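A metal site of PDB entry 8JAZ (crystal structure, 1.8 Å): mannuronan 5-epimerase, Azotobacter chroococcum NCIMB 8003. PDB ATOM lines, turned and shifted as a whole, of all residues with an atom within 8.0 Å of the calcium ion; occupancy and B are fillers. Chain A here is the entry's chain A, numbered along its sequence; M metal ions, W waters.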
ATOM      1  N   THR A  36      15.101  30.152   5.240  1.00  0.00           N
ATOM      2  CA  THR A  36      13.723  29.691   5.087  1.00  0.00           C
ATOM      3  C   THR A  36      13.577  28.327   5.740  1.00  0.00           C
ATOM      4  O   THR A  36      14.329  27.397   5.438  1.00  0.00           O
ATOM      5  CB  THR A  36      13.340  29.622   3.611  1.00  0.00           C
ATOM      6  OG1 THR A  36      13.284  30.954   3.073  1.00  0.00           O
ATOM      7  CG2 THR A  36      11.976  28.966   3.448  1.00  0.00           C
ATOM      8  N   ARG A  38      11.202  25.351   5.747  1.00  0.00           N
ATOM      9  CA  ARG A  38      10.194  24.846   4.823  1.00  0.00           C
ATOM     10  C   ARG A  38       9.486  23.649   5.428  1.00  0.00           C
ATOM     11  O   ARG A  38      10.122  22.748   5.984  1.00  0.00           O
ATOM     12  CB  ARG A  38      10.826  24.465   3.482  1.00  0.00           C
ATOM     13  CG  ARG A  38       9.822  24.384   2.345  1.00  0.00           C
ATOM     14  CD  ARG A  38      10.504  24.501   0.989  1.00  0.00           C
ATOM     15  NE  ARG A  38      11.184  25.783   0.834  1.00  0.00           N
ATOM     16  CZ  ARG A  38      10.626  26.865   0.301  1.00  0.00           C
ATOM     17  NH1 ARG A  38       9.384  26.856  -0.130  1.00  0.00           N
ATOM     18  NH2 ARG A  38      11.344  27.983   0.206  1.00  0.00           N
ATOM     19  N   LEU A  39       8.155  23.642   5.311  1.00  0.00           N
ATOM     20  CA  LEU A  39       7.332  22.512   5.723  1.00  0.00           C
ATOM     21  C   LEU A  39       6.618  21.976   4.502  1.00  0.00           C
ATOM     22  O   LEU A  39       5.930  22.720   3.798  1.00  0.00           O
ATOM     23  CB  LEU A  39       6.314  22.927   6.796  1.00  0.00           C
ATOM     24  CG  LEU A  39       6.784  23.712   8.032  1.00  0.00           C
ATOM     25  CD1 LEU A  39       6.827  25.205   7.754  1.00  0.00           C
ATOM     26  CD2 LEU A  39       5.903  23.397   9.221  1.00  0.00           C
ATOM     27  N   MET A  65       9.080  31.246   7.592  1.00  0.00           N
ATOM     28  CA  MET A  65       8.463  29.927   7.552  1.00  0.00           C
ATOM     29  C   MET A  65       7.594  29.827   6.300  1.00  0.00           C
ATOM     30  O   MET A  65       6.767  30.700   6.049  1.00  0.00           O
ATOM     31  CB  MET A  65       7.629  29.673   8.809  1.00  0.00           C
ATOM     32  CG  MET A  65       8.453  29.574  10.081  1.00  0.00           C
ATOM     33  SD  MET A  65       7.407  29.358  11.530  1.00  0.00           S
ATOM     34  CE  MET A  65       7.226  27.577  11.526  1.00  0.00           C
ATOM     35  N   ASP A  66       7.794  28.755   5.535  1.00  0.00           N
ATOM     36  CA  ASP A  66       7.186  28.627   4.211  1.00  0.00           C
ATOM     37  C   ASP A  66       6.657  27.212   4.046  1.00  0.00           C
ATOM     38  O   ASP A  66       7.448  26.265   3.971  1.00  0.00           O
ATOM     39  CB  ASP A  66       8.204  28.964   3.117  1.00  0.00           C
ATOM     40  CG  ASP A  66       7.556  29.264   1.774  1.00  0.00           C
ATOM     41  OD1 ASP A  66       6.710  28.458   1.323  1.00  0.00           O
ATOM     42  OD2 ASP A  66       7.903  30.293   1.162  1.00  0.00           O
ATOM     43  N   GLY A  67       5.339  27.059   3.991  1.00  0.00           N
ATOM     44  CA  GLY A  67       4.716  25.765   3.841  1.00  0.00           C
ATOM     45  C   GLY A  67       4.347  25.445   2.398  1.00  0.00           C
ATOM     46  O   GLY A  67       4.747  26.134   1.453  1.00  0.00           O
ATOM     47  N   ALA A  68       3.572  24.375   2.234  1.00  0.00           N
ATOM     48  CA  ALA A  68       3.146  23.907   0.925  1.00  0.00           C
ATOM     49  C   ALA A  68       1.852  24.552   0.441  1.00  0.00           C
ATOM     50  O   ALA A  68       1.400  24.254  -0.665  1.00  0.00           O
ATOM     51  CB  ALA A  68       2.983  22.384   0.930  1.00  0.00           C
ATOM     52  N   GLY A  69       1.241  25.426   1.239  1.00  0.00           N
ATOM     53  CA  GLY A  69       0.012  26.072   0.835  1.00  0.00           C
ATOM     54  C   GLY A  69      -1.079  26.005   1.888  1.00  0.00           C
ATOM     55  O   GLY A  69      -1.052  25.150   2.771  1.00  0.00           O
ATOM     56  N   MET A  70      -2.035  26.935   1.803  1.00  0.00           N
ATOM     57  CA  MET A  70      -3.174  26.919   2.715  1.00  0.00           C
ATOM     58  C   MET A  70      -3.948  25.613   2.581  1.00  0.00           C
ATOM     59  O   MET A  70      -4.264  25.175   1.464  1.00  0.00           O
ATOM     60  CB  MET A  70      -4.094  28.096   2.426  1.00  0.00           C
ATOM     61  CG  MET A  70      -3.383  29.430   2.277  1.00  0.00           C
ATOM     62  SD  MET A  70      -4.479  30.755   1.731  1.00  0.00           S
ATOM     63  CE  MET A  70      -6.072  29.952   1.808  1.00  0.00           C
ATOM     64  N   THR A  73      -0.245  22.642   4.110  1.00  0.00           N
ATOM     65  CA  THR A  73       0.559  22.684   5.326  1.00  0.00           C
ATOM     66  C   THR A  73      -0.288  23.302   6.429  1.00  0.00           C
ATOM     67  O   THR A  73      -0.666  24.477   6.341  1.00  0.00           O
ATOM     68  CB  THR A  73       1.848  23.484   5.123  1.00  0.00           C
ATOM     69  OG1 THR A  73       2.683  22.820   4.164  1.00  0.00           O
ATOM     70  CG2 THR A  73       2.600  23.607   6.443  1.00  0.00           C
ATOM     71  N   ARG A 103       4.597  32.187   5.144  1.00  0.00           N
ATOM     72  CA  ARG A 103       4.054  32.005   3.807  1.00  0.00           C
ATOM     73  C   ARG A 103       3.468  30.624   3.651  1.00  0.00           C
ATOM     74  O   ARG A 103       3.986  29.642   4.195  1.00  0.00           O
ATOM     75  CB  ARG A 103       5.130  32.223   2.727  1.00  0.00           C
ATOM     76  CG  ARG A 103       5.785  33.589   2.710  1.00  0.00           C
ATOM     77  CD  ARG A 103       6.548  33.792   1.416  1.00  0.00           C
ATOM     78  NE  ARG A 103       7.777  34.552   1.598  1.00  0.00           N
ATOM     79  CZ  ARG A 103       8.939  34.028   1.978  1.00  0.00           C
ATOM     80  NH1 ARG A 103       9.066  32.736   2.213  1.00  0.00           N
ATOM     81  NH2 ARG A 103       9.999  34.827   2.108  1.00  0.00           N
ATOM     82  N   ASP A 104       2.358  30.546   2.910  1.00  0.00           N
ATOM     83  CA  ASP A 104       1.858  29.295   2.330  1.00  0.00           C
ATOM     84  C   ASP A 104       1.554  28.241   3.394  1.00  0.00           C
ATOM     85  O   ASP A 104       1.984  27.085   3.297  1.00  0.00           O
ATOM     86  CB  ASP A 104       2.862  28.737   1.306  1.00  0.00           C
ATOM     87  CG  ASP A 104       2.927  29.569   0.045  1.00  0.00           C
ATOM     88  OD1 ASP A 104       1.979  30.344  -0.217  1.00  0.00           O
ATOM     89  OD2 ASP A 104       3.924  29.442  -0.694  1.00  0.00           O
ATOM     90  N   LEU A 105       0.787  28.624   4.414  1.00  0.00           N
ATOM     91  CA  LEU A 105       0.457  27.663   5.464  1.00  0.00           C
ATOM     92  C   LEU A 105      -0.867  28.032   6.114  1.00  0.00           C
ATOM     93  O   LEU A 105      -1.418  29.117   5.924  1.00  0.00           O
ATOM     94  CB  LEU A 105       1.578  27.576   6.514  1.00  0.00           C
ATOM     95  CG  LEU A 105       2.139  28.868   7.129  1.00  0.00           C
ATOM     96  CD1 LEU A 105       1.308  29.333   8.308  1.00  0.00           C
ATOM     97  CD2 LEU A 105       3.595  28.668   7.536  1.00  0.00           C
ATOM     98  N   ARG A 140      -0.220  34.672   1.790  1.00  0.00           N
ATOM     99  CA  ARG A 140      -0.928  33.443   1.446  1.00  0.00           C
ATOM    100  C   ARG A 140      -1.019  32.519   2.658  1.00  0.00           C
ATOM    101  O   ARG A 140      -0.677  31.338   2.592  1.00  0.00           O
ATOM    102  CB  ARG A 140      -0.259  32.748   0.261  1.00  0.00           C
ATOM    103  CG  ARG A 140      -0.268  33.584  -1.016  1.00  0.00           C
ATOM    104  CD  ARG A 140       0.535  32.919  -2.121  1.00  0.00           C
ATOM    105  NE  ARG A 140       1.929  32.743  -1.734  1.00  0.00           N
ATOM    106  CZ  ARG A 140       2.862  33.676  -1.866  1.00  0.00           C
ATOM    107  NH1 ARG A 140       2.579  34.872  -2.382  1.00  0.00           N
ATOM    108  NH2 ARG A 140       4.099  33.419  -1.471  1.00  0.00           N
HETATM  109 CA    CA M   1       5.548  27.364  -0.341  1.00  0.00          CA
HETATM  110  O   HOH W   1       3.820  26.533  -1.794  1.00  0.00           O
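The guanidinium group of Arg 38 lies within salt-bridge range of the side-chain carboxylate of Asp 66, 3.96 Å away.
The guanidinium group (NH1) of Arg 103 is in salt-bridge range of the side-chain carboxylate (OD2) of Asp 66.
The backbone NH of Leu 39 is in hydrogen-bond range of the backbone carbonyl oxygen of Asp 66, at 3.0 Å.
The backbone NH (N) of Gly 67 is in hydrogen-bond range of the backbone carbonyl oxygen (O) of Arg 103 (2.9 Å).
The backbone carbonyl oxygen of Asp 104 lies within hydrogen-bond range of the backbone NH of Ala 68, at 3.3 Å.
O of Asp 104 lies within hydrogen-bond range of N of Gly 69 (2.7 Å).
OD1 of Asp 104 lies within salt-bridge range of NE of Arg 140 (2.8 Å).
Residues that only touch the calcium ion: Arg 38 (3.9 Å).
Four residues have an atom within 4 Å of the calcium ion: Arg 38, Asp 66, Gly 67 and Asp 104.
Along chain A the residues within 4 Å of the calcium ion span positions 38 to 104.
The nearest printed residue that does not touch the calcium ion is Ala 68 (4.4 Å).
OD1 of Asp 66 binds the calcium ion.
The calcium ion is bound by O of Gly 67, at 2.3 Å.
Water W1 binds the calcium ion, 2.4 Å away.
OD2 of Asp 104 is bound to the calcium ion, 2.7 Å away.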
